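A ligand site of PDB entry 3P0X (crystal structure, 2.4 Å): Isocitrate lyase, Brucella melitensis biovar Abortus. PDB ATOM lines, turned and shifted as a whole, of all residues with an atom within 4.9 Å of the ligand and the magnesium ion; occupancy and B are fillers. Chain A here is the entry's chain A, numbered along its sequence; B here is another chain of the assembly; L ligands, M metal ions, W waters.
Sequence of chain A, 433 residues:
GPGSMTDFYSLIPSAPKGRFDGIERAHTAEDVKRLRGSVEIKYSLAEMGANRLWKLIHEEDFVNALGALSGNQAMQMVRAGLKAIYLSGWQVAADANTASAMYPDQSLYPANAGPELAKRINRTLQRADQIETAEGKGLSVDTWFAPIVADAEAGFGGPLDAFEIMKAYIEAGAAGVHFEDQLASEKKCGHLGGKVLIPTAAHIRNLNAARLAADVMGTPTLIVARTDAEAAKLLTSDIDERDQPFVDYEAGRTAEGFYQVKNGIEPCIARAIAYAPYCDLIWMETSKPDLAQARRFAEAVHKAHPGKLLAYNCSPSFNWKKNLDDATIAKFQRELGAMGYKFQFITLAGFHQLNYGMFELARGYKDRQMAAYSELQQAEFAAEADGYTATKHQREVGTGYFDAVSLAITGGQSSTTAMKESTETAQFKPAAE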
ATOM      1  N   TYR A  86      10.382 -21.240  23.108  1.00  0.00           N
ATOM      2  CA  TYR A  86       8.982 -21.406  23.501  1.00  0.00           C
ATOM      3  C   TYR A  86       8.320 -22.244  22.424  1.00  0.00           C
ATOM      4  O   TYR A  86       8.633 -22.119  21.239  1.00  0.00           O
ATOM      5  CB  TYR A  86       8.241 -20.068  23.662  1.00  0.00           C
ATOM      6  CG  TYR A  86       6.782 -20.282  23.977  1.00  0.00           C
ATOM      7  CD1 TYR A  86       6.384 -20.781  25.214  1.00  0.00           C
ATOM      8  CD2 TYR A  86       5.794 -20.018  23.044  1.00  0.00           C
ATOM      9  CE1 TYR A  86       5.072 -20.999  25.505  1.00  0.00           C
ATOM     10  CE2 TYR A  86       4.469 -20.230  23.332  1.00  0.00           C
ATOM     11  CZ  TYR A  86       4.114 -20.742  24.566  1.00  0.00           C
ATOM     12  OH  TYR A  86       2.802 -20.947  24.852  1.00  0.00           O
ATOM     13  N   SER A  88       4.616 -23.068  21.152  1.00  0.00           N
ATOM     14  CA  SER A  88       3.251 -22.607  21.151  1.00  0.00           C
ATOM     15  C   SER A  88       2.350 -23.727  20.667  1.00  0.00           C
ATOM     16  O   SER A  88       2.672 -24.390  19.689  1.00  0.00           O
ATOM     17  CB  SER A  88       3.112 -21.441  20.184  1.00  0.00           C
ATOM     18  OG  SER A  88       1.805 -21.360  19.638  1.00  0.00           O
ATOM     19  N   GLY A  89       1.209 -23.904  21.347  1.00  0.00           N
ATOM     20  CA  GLY A  89       0.194 -24.851  20.898  1.00  0.00           C
ATOM     21  C   GLY A  89      -0.599 -24.280  19.729  1.00  0.00           C
ATOM     22  O   GLY A  89      -1.048 -25.022  18.838  1.00  0.00           O
ATOM     23  N   TRP A  90      -0.756 -22.973  19.751  1.00  0.00           N
ATOM     24  CA  TRP A  90      -1.372 -22.225  18.669  1.00  0.00           C
ATOM     25  C   TRP A  90      -0.641 -22.529  17.356  1.00  0.00           C
ATOM     26  O   TRP A  90      -1.286 -22.816  16.346  1.00  0.00           O
ATOM     27  CB  TRP A  90      -1.354 -20.715  18.999  1.00  0.00           C
ATOM     28  CG  TRP A  90      -2.211 -19.847  18.084  1.00  0.00           C
ATOM     29  CD1 TRP A  90      -3.387 -19.216  18.402  1.00  0.00           C
ATOM     30  CD2 TRP A  90      -1.928 -19.495  16.723  1.00  0.00           C
ATOM     31  NE1 TRP A  90      -3.868 -18.530  17.304  1.00  0.00           N
ATOM     32  CE2 TRP A  90      -2.983 -18.678  16.268  1.00  0.00           C
ATOM     33  CE3 TRP A  90      -0.880 -19.793  15.845  1.00  0.00           C
ATOM     34  CZ2 TRP A  90      -3.024 -18.157  14.979  1.00  0.00           C
ATOM     35  CZ3 TRP A  90      -0.928 -19.285  14.564  1.00  0.00           C
ATOM     36  CH2 TRP A  90      -1.990 -18.468  14.139  1.00  0.00           C
ATOM     37  N   ASP A 105      -6.903 -22.470  17.326  1.00  0.00           N
ATOM     38  CA  ASP A 105      -6.267 -22.839  18.571  1.00  0.00           C
ATOM     39  C   ASP A 105      -7.325 -23.326  19.539  1.00  0.00           C
ATOM     40  O   ASP A 105      -7.650 -22.635  20.485  1.00  0.00           O
ATOM     41  CB  ASP A 105      -5.511 -21.616  19.087  1.00  0.00           C
ATOM     42  CG  ASP A 105      -4.661 -21.914  20.296  1.00  0.00           C
ATOM     43  OD1 ASP A 105      -4.170 -23.064  20.463  1.00  0.00           O
ATOM     44  OD2 ASP A 105      -4.496 -20.967  21.072  1.00  0.00           O
ATOM     45  N   ASP A 151       3.638 -25.750  25.513  1.00  0.00           N
ATOM     46  CA  ASP A 151       2.216 -25.621  25.755  1.00  0.00           C
ATOM     47  C   ASP A 151       1.527 -27.010  25.829  1.00  0.00           C
ATOM     48  O   ASP A 151       1.465 -27.727  24.827  1.00  0.00           O
ATOM     49  CB  ASP A 151       1.662 -24.812  24.565  1.00  0.00           C
ATOM     50  CG  ASP A 151       0.238 -24.373  24.733  1.00  0.00           C
ATOM     51  OD1 ASP A 151      -0.437 -24.836  25.643  1.00  0.00           O
ATOM     52  OD2 ASP A 151      -0.202 -23.539  23.936  1.00  0.00           O
ATOM     53  N   GLU A 153      -1.606 -26.939  26.734  1.00  0.00           N
ATOM     54  CA  GLU A 153      -2.977 -26.427  26.652  1.00  0.00           C
ATOM     55  C   GLU A 153      -3.759 -26.694  27.942  1.00  0.00           C
ATOM     56  O   GLU A 153      -3.352 -26.223  29.029  1.00  0.00           O
ATOM     57  CB  GLU A 153      -3.632 -26.955  25.370  1.00  0.00           C
ATOM     58  CG  GLU A 153      -2.750 -26.626  24.147  1.00  0.00           C
ATOM     59  CD  GLU A 153      -3.422 -26.771  22.792  1.00  0.00           C
ATOM     60  OE1 GLU A 153      -4.508 -27.399  22.705  1.00  0.00           O
ATOM     61  OE2 GLU A 153      -2.844 -26.285  21.803  1.00  0.00           O
ATOM     62  N   HIS A 178       3.369 -25.880  30.360  1.00  0.00           N
ATOM     63  CA  HIS A 178       2.323 -25.064  30.908  1.00  0.00           C
ATOM     64  C   HIS A 178       0.945 -25.616  30.692  1.00  0.00           C
ATOM     65  O   HIS A 178       0.660 -26.196  29.655  1.00  0.00           O
ATOM     66  CB  HIS A 178       2.467 -23.567  30.467  1.00  0.00           C
ATOM     67  CG  HIS A 178       2.081 -23.229  29.055  1.00  0.00           C
ATOM     68  ND1 HIS A 178       0.775 -23.162  28.640  1.00  0.00           N
ATOM     69  CD2 HIS A 178       2.823 -22.749  28.033  1.00  0.00           C
ATOM     70  CE1 HIS A 178       0.724 -22.735  27.388  1.00  0.00           C
ATOM     71  NE2 HIS A 178       1.959 -22.478  26.993  1.00  0.00           N
ATOM     72  N   GLU A 180      -3.339 -24.717  31.490  1.00  0.00           N
ATOM     73  CA  GLU A 180      -4.244 -23.611  31.703  1.00  0.00           C
ATOM     74  C   GLU A 180      -5.592 -24.093  32.243  1.00  0.00           C
ATOM     75  O   GLU A 180      -5.986 -25.223  32.040  1.00  0.00           O
ATOM     76  CB  GLU A 180      -4.417 -22.845  30.402  1.00  0.00           C
ATOM     77  CG  GLU A 180      -5.247 -23.560  29.332  1.00  0.00           C
ATOM     78  CD  GLU A 180      -4.815 -23.207  27.910  1.00  0.00           C
ATOM     79  OE1 GLU A 180      -3.653 -22.742  27.744  1.00  0.00           O
ATOM     80  OE2 GLU A 180      -5.639 -23.402  26.956  1.00  0.00           O
ATOM     81  N   LYS A 187     -11.650 -25.562  24.646  1.00  0.00           N
ATOM     82  CA  LYS A 187     -10.432 -24.743  24.672  1.00  0.00           C
ATOM     83  C   LYS A 187     -10.363 -23.672  23.556  1.00  0.00           C
ATOM     84  O   LYS A 187     -10.752 -23.910  22.400  1.00  0.00           O
ATOM     85  CB  LYS A 187      -9.174 -25.639  24.569  1.00  0.00           C
ATOM     86  CG  LYS A 187      -7.831 -24.891  24.835  1.00  0.00           C
ATOM     87  CD  LYS A 187      -7.177 -24.334  23.534  1.00  0.00           C
ATOM     88  CE  LYS A 187      -5.737 -23.824  23.744  1.00  0.00           C
ATOM     89  NZ  LYS A 187      -5.654 -22.524  24.461  1.00  0.00           N
ATOM     90  N   LYS A 188      -9.856 -22.489  23.916  1.00  0.00           N
ATOM     91  CA  LYS A 188      -9.615 -21.415  22.947  1.00  0.00           C
ATOM     92  C   LYS A 188      -8.255 -20.826  23.144  1.00  0.00           C
ATOM     93  O   LYS A 188      -7.640 -20.981  24.213  1.00  0.00           O
ATOM     94  CB  LYS A 188     -10.609 -20.261  23.093  1.00  0.00           C
ATOM     95  CG  LYS A 188     -12.069 -20.636  23.181  1.00  0.00           C
ATOM     96  CD  LYS A 188     -12.648 -21.076  21.877  1.00  0.00           C
ATOM     97  CE  LYS A 188     -14.157 -21.263  21.991  1.00  0.00           C
ATOM     98  NZ  LYS A 188     -14.577 -21.966  23.240  1.00  0.00           N
ATOM     99  N   CYS A 189      -7.805 -20.104  22.134  1.00  0.00           N
ATOM    100  CA  CYS A 189      -6.723 -19.171  22.311  1.00  0.00           C
ATOM    101  C   CYS A 189      -7.117 -18.232  23.445  1.00  0.00           C
ATOM    102  O   CYS A 189      -8.288 -17.820  23.536  1.00  0.00           O
ATOM    103  CB  CYS A 189      -6.503 -18.377  21.013  1.00  0.00           C
ATOM    104  SG  CYS A 189      -5.304 -17.058  21.092  1.00  0.00           S
ATOM    105  N   GLY A 190      -6.153 -17.901  24.300  1.00  0.00           N
ATOM    106  CA  GLY A 190      -6.395 -16.977  25.402  1.00  0.00           C
ATOM    107  C   GLY A 190      -7.034 -15.646  24.999  1.00  0.00           C
ATOM    108  O   GLY A 190      -7.825 -15.070  25.758  1.00  0.00           O
ATOM    109  N   HIS A 191      -6.711 -15.172  23.796  1.00  0.00           N
ATOM    110  CA  HIS A 191      -7.193 -13.864  23.328  1.00  0.00           C
ATOM    111  C   HIS A 191      -8.415 -13.924  22.397  1.00  0.00           C
ATOM    112  O   HIS A 191      -8.748 -12.930  21.750  1.00  0.00           O
ATOM    113  CB  HIS A 191      -6.029 -13.123  22.682  1.00  0.00           C
ATOM    114  CG  HIS A 191      -4.860 -12.987  23.609  1.00  0.00           C
ATOM    115  ND1 HIS A 191      -3.684 -13.668  23.425  1.00  0.00           N
ATOM    116  CD2 HIS A 191      -4.734 -12.320  24.778  1.00  0.00           C
ATOM    117  CE1 HIS A 191      -2.855 -13.388  24.417  1.00  0.00           C
ATOM    118  NE2 HIS A 191      -3.475 -12.576  25.264  1.00  0.00           N
ATOM    119  N   ARG A 226      -1.228 -21.467  34.222  1.00  0.00           N
ATOM    120  CA  ARG A 226      -1.806 -20.329  33.542  1.00  0.00           C
ATOM    121  C   ARG A 226      -3.274 -20.206  33.930  1.00  0.00           C
ATOM    122  O   ARG A 226      -3.961 -21.217  34.009  1.00  0.00           O
ATOM    123  CB  ARG A 226      -1.677 -20.546  32.055  1.00  0.00           C
ATOM    124  CG  ARG A 226      -2.653 -19.758  31.226  1.00  0.00           C
ATOM    125  CD  ARG A 226      -2.310 -19.859  29.757  1.00  0.00           C
ATOM    126  NE  ARG A 226      -3.487 -19.582  28.937  1.00  0.00           N
ATOM    127  CZ  ARG A 226      -3.449 -19.468  27.626  1.00  0.00           C
ATOM    128  NH1 ARG A 226      -2.301 -19.624  26.991  1.00  0.00           N
ATOM    129  NH2 ARG A 226      -4.554 -19.221  26.943  1.00  0.00           N
ATOM    130  N   TRP A 283       1.197 -17.638  35.528  1.00  0.00           N
ATOM    131  CA  TRP A 283       1.000 -16.852  34.327  1.00  0.00           C
ATOM    132  C   TRP A 283      -0.475 -16.479  34.224  1.00  0.00           C
ATOM    133  O   TRP A 283      -1.359 -17.351  34.294  1.00  0.00           O
ATOM    134  CB  TRP A 283       1.489 -17.659  33.114  1.00  0.00           C
ATOM    135  CG  TRP A 283       1.031 -17.212  31.741  1.00  0.00           C
ATOM    136  CD1 TRP A 283       0.593 -15.985  31.367  1.00  0.00           C
ATOM    137  CD2 TRP A 283       1.039 -18.003  30.544  1.00  0.00           C
ATOM    138  NE1 TRP A 283       0.295 -15.962  30.022  1.00  0.00           N
ATOM    139  CE2 TRP A 283       0.553 -17.191  29.501  1.00  0.00           C
ATOM    140  CE3 TRP A 283       1.383 -19.336  30.261  1.00  0.00           C
ATOM    141  CZ2 TRP A 283       0.422 -17.650  28.184  1.00  0.00           C
ATOM    142  CZ3 TRP A 283       1.258 -19.790  28.956  1.00  0.00           C
ATOM    143  CH2 TRP A 283       0.785 -18.944  27.929  1.00  0.00           C
ATOM    144  N   GLU A 285      -2.997 -14.783  31.566  1.00  0.00           N
ATOM    145  CA  GLU A 285      -3.296 -14.198  30.252  1.00  0.00           C
ATOM    146  C   GLU A 285      -3.930 -12.817  30.414  1.00  0.00           C
ATOM    147  O   GLU A 285      -4.736 -12.621  31.314  1.00  0.00           O
ATOM    148  CB  GLU A 285      -4.224 -15.085  29.429  1.00  0.00           C
ATOM    149  CG  GLU A 285      -3.516 -16.225  28.756  1.00  0.00           C
ATOM    150  CD  GLU A 285      -2.902 -15.839  27.431  1.00  0.00           C
ATOM    151  OE1 GLU A 285      -1.757 -15.333  27.415  1.00  0.00           O
ATOM    152  OE2 GLU A 285      -3.562 -16.031  26.399  1.00  0.00           O
ATOM    153  N   ASN A 313       3.011 -13.460  28.728  1.00  0.00           N
ATOM    154  CA  ASN A 313       2.866 -13.598  27.271  1.00  0.00           C
ATOM    155  C   ASN A 313       2.898 -12.264  26.567  1.00  0.00           C
ATOM    156  O   ASN A 313       1.931 -11.516  26.600  1.00  0.00           O
ATOM    157  CB  ASN A 313       1.558 -14.317  26.917  1.00  0.00           C
ATOM    158  CG  ASN A 313       1.308 -14.396  25.384  1.00  0.00           C
ATOM    159  OD1 ASN A 313       2.165 -14.053  24.552  1.00  0.00           O
ATOM    160  ND2 ASN A 313       0.125 -14.897  25.015  1.00  0.00           N
ATOM    161  N   SER A 315       2.141 -11.096  23.608  1.00  0.00           N
ATOM    162  CA  SER A 315       1.351 -11.658  22.524  1.00  0.00           C
ATOM    163  C   SER A 315       1.306 -10.826  21.239  1.00  0.00           C
ATOM    164  O   SER A 315       1.089  -9.617  21.293  1.00  0.00           O
ATOM    165  CB  SER A 315      -0.094 -11.851  22.985  1.00  0.00           C
ATOM    166  OG  SER A 315      -0.853 -12.478  21.947  1.00  0.00           O
ATOM    167  N   PRO A 316       1.467 -11.474  20.069  1.00  0.00           N
ATOM    168  CA  PRO A 316       1.191 -10.855  18.790  1.00  0.00           C
ATOM    169  C   PRO A 316      -0.279 -10.658  18.537  1.00  0.00           C
ATOM    170  O   PRO A 316      -0.636  -9.961  17.602  1.00  0.00           O
ATOM    171  CB  PRO A 316       1.748 -11.867  17.799  1.00  0.00           C
ATOM    172  CG  PRO A 316       2.859 -12.461  18.530  1.00  0.00           C
ATOM    173  CD  PRO A 316       2.295 -12.662  19.894  1.00  0.00           C
ATOM    174  N   SER A 317      -1.132 -11.257  19.374  1.00  0.00           N
ATOM    175  CA  SER A 317      -2.563 -10.924  19.377  1.00  0.00           C
ATOM    176  C   SER A 317      -2.811  -9.467  19.817  1.00  0.00           C
ATOM    177  O   SER A 317      -3.935  -8.978  19.729  1.00  0.00           O
ATOM    178  CB  SER A 317      -3.385 -11.908  20.252  1.00  0.00           C
ATOM    179  OG  SER A 317      -3.198 -13.294  19.899  1.00  0.00           O
ATOM    180  N   THR A 347       4.600 -15.669  21.907  1.00  0.00           N
ATOM    181  CA  THR A 347       4.009 -16.934  21.512  1.00  0.00           C
ATOM    182  C   THR A 347       4.073 -17.208  19.997  1.00  0.00           C
ATOM    183  O   THR A 347       4.548 -18.269  19.576  1.00  0.00           O
ATOM    184  CB  THR A 347       2.539 -16.959  21.899  1.00  0.00           C
ATOM    185  OG1 THR A 347       1.923 -15.774  21.394  1.00  0.00           O
ATOM    186  CG2 THR A 347       2.355 -17.025  23.415  1.00  0.00           C
ATOM    187  N   LEU A 348       3.555 -16.286  19.191  1.00  0.00           N
ATOM    188  CA  LEU A 348       3.346 -16.553  17.763  1.00  0.00           C
ATOM    189  C   LEU A 348       4.404 -15.936  16.837  1.00  0.00           C
ATOM    190  O   LEU A 348       4.138 -15.714  15.664  1.00  0.00           O
ATOM    191  CB  LEU A 348       1.968 -16.107  17.301  1.00  0.00           C
ATOM    192  CG  LEU A 348       0.766 -16.558  18.146  1.00  0.00           C
ATOM    193  CD1 LEU A 348      -0.539 -16.104  17.460  1.00  0.00           C
ATOM    194  CD2 LEU A 348       0.778 -18.078  18.394  1.00  0.00           C
ATOM    195  N   GLN B 394      -5.935 -15.201  13.602  1.00  0.00           N
ATOM    196  CA  GLN B 394      -7.032 -16.081  13.975  1.00  0.00           C
ATOM    197  C   GLN B 394      -7.834 -16.488  12.738  1.00  0.00           C
ATOM    198  O   GLN B 394      -8.163 -17.665  12.538  1.00  0.00           O
ATOM    199  CB  GLN B 394      -7.936 -15.424  15.018  1.00  0.00           C
ATOM    200  CG  GLN B 394      -7.192 -14.841  16.266  1.00  0.00           C
ATOM    201  CD  GLN B 394      -6.502 -15.882  17.155  1.00  0.00           C
ATOM    202  OE1 GLN B 394      -6.337 -17.059  16.790  1.00  0.00           O
ATOM    203  NE2 GLN B 394      -6.070 -15.437  18.355  1.00  0.00           N
HETATM  204  C1  LIG L   1       0.051 -20.318  22.307  1.00  0.00           C
HETATM  205  O1  LIG L   1       0.930 -19.847  21.557  1.00  0.00           O
HETATM  206  O2  LIG L   1      -0.399 -21.493  22.218  1.00  0.00           O
HETATM  207  C2  LIG L   1      -0.535 -19.442  23.393  1.00  0.00           C
HETATM  208  O3  LIG L   1      -0.998 -20.361  24.389  1.00  0.00           O
HETATM  209  C3  LIG L   1      -1.639 -18.504  22.809  1.00  0.00           C
HETATM  210  C4  LIG L   1      -1.075 -17.429  21.823  1.00  0.00           C
HETATM  211  C5  LIG L   1      -1.432 -15.942  21.953  1.00  0.00           C
HETATM  212  O4  LIG L   1      -2.571 -15.549  21.582  1.00  0.00           O
HETATM  213  O5  LIG L   1      -0.535 -15.132  22.336  1.00  0.00           O
HETATM  214  C6  LIG L   1      -2.468 -17.984  23.947  1.00  0.00           C
HETATM  215  O6  LIG L   1      -3.518 -18.590  24.238  1.00  0.00           O
HETATM  216  O7  LIG L   1      -2.080 -17.003  24.583  1.00  0.00           O
HETATM  217 MG    MG M   1      -1.593 -22.159  23.780  1.00  0.00          MG
HETATM  218  O   HOH W   1      -3.441 -21.113  23.385  1.00  0.00           O
HETATM  219  O   HOH W   2      -2.268 -23.030  25.534  1.00  0.00           O
HETATM  220  O   HOH W   3      -2.668 -23.411  22.330  1.00  0.00           O
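OE2 of Glu 285 lies close to O7 of the ligand, 2.5 Å away. An oxygen (O1) of the ligand lies within hydrogen-bond range of the side-chain hydroxyl (OG) of Ser 88, 2.6 Å away. OG of Ser 315 is in hydrogen-bond range of O5 of the ligand (2.7 Å). The side-chain hydroxyl (OG1) of Thr 347 is in hydrogen-bond range of an oxygen (O5) of the ligand (2.7 Å). O6 of the ligand lies within hydrogen-bond range of N of Gly 190. ND2 of Asn 313 is in hydrogen-bond range of O5 of the ligand (2.8 Å). A ring nitrogen (ND1) of His 191 sits at hydrogen-bond distance from an oxygen (O4) of the ligand, 2.9 Å away. An oxygen (O4) of the ligand lies within hydrogen-bond range of the side-chain hydroxyl (OG) of Ser 317 (2.9 Å). The backbone NH (N) of Trp 90 lies close to an oxygen (O2) of the ligand, at 2.9 Å. NH2 of Arg 226 lies within salt-bridge range of O6 of the ligand. The backbone NH (N) of Gly 89 sits close to an oxygen (O2) of the ligand. The side-chain sulfur of Cys 189 lies within hydrogen-bond range of an oxygen (O4) of the ligand (3.2 Å).
The backbone NH (N) of Gly 89 lies close to the side-chain carboxylate (OD2) of Asp 151, at 3.0 Å. The side-chain carboxylate (OD1) of Asp 151 sits at hydrogen-bond distance from the backbone NH (N) of Glu 153, at 2.6 Å. ND2 of Asn 313 lies within hydrogen-bond range of OE1 of Glu 285 (3.1 Å). The side-chain carboxylate (OE1) of Glu 285 lies close to the indole nitrogen (NE1) of Trp 283 (3.4 Å). OG of Ser 315 is in hydrogen-bond range of N of Ser 317 (2.9 Å). SG of Cys 189 lies close to N of His 191, 3.6 Å away. The guanidinium group (NE) of Arg 226 is in salt-bridge range of the side-chain carboxylate (OE1) of Glu 180 (3.4 Å). The backbone NH of Cys 189 sits at hydrogen-bond distance from the backbone carbonyl oxygen of Asp 105.
Tyr 86 touches the ligand (OH to C1, 3.8 Å). Leu 348 touches the ligand. Hydrophobic or aromatic side chains within 4 Å of the ligand: Tyr 86, Trp 90, His 191 and Leu 348. Within 4 Å of the ligand: Tyr 86, Ser 88, Gly 89, Trp 90, Asp 151, Cys 189, Gly 190, His 191, Arg 226, Glu 285, Asn 313, Ser 315, Ser 317, Thr 347 and Leu 348. Along chain A the residues within 4 Å of the ligand span positions 86 to 348. The nearest printed residue that does not touch the ligand is Asp 105 (4.1 Å).
Within 4 Å of the magnesium ion: Asp 151.
The magnesium ion is bound by the side-chain carboxylate (OD2) of Asp 151 (2.0 Å), an oxygen (O3) of the ligand (2.0 Å), water W2 (2.1 Å), an oxygen (O2) of the ligand (2.1 Å), water W1 (2.2 Å) and water W3 (2.2 Å). The magnesium ion has six donor atoms within binding distance.
Water W3 lies within hydrogen-bond range of OD1 of Asp 105 (2.4 Å), OE2 of Glu 153 (2.9 Å) and N of Trp 90 (3.2 Å). Water W2 lies within hydrogen-bond range of the side-chain carboxylate (OD1) of Asp 151 and the side-chain carboxylate (OE1) of Glu 180. Water W1 lies within hydrogen-bond range of the side-chain carboxylate of Asp 105 (2.5 Å), an oxygen (O6) of the ligand (2.7 Å) and the side-chain amino group of Lys 187 (2.8 Å).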
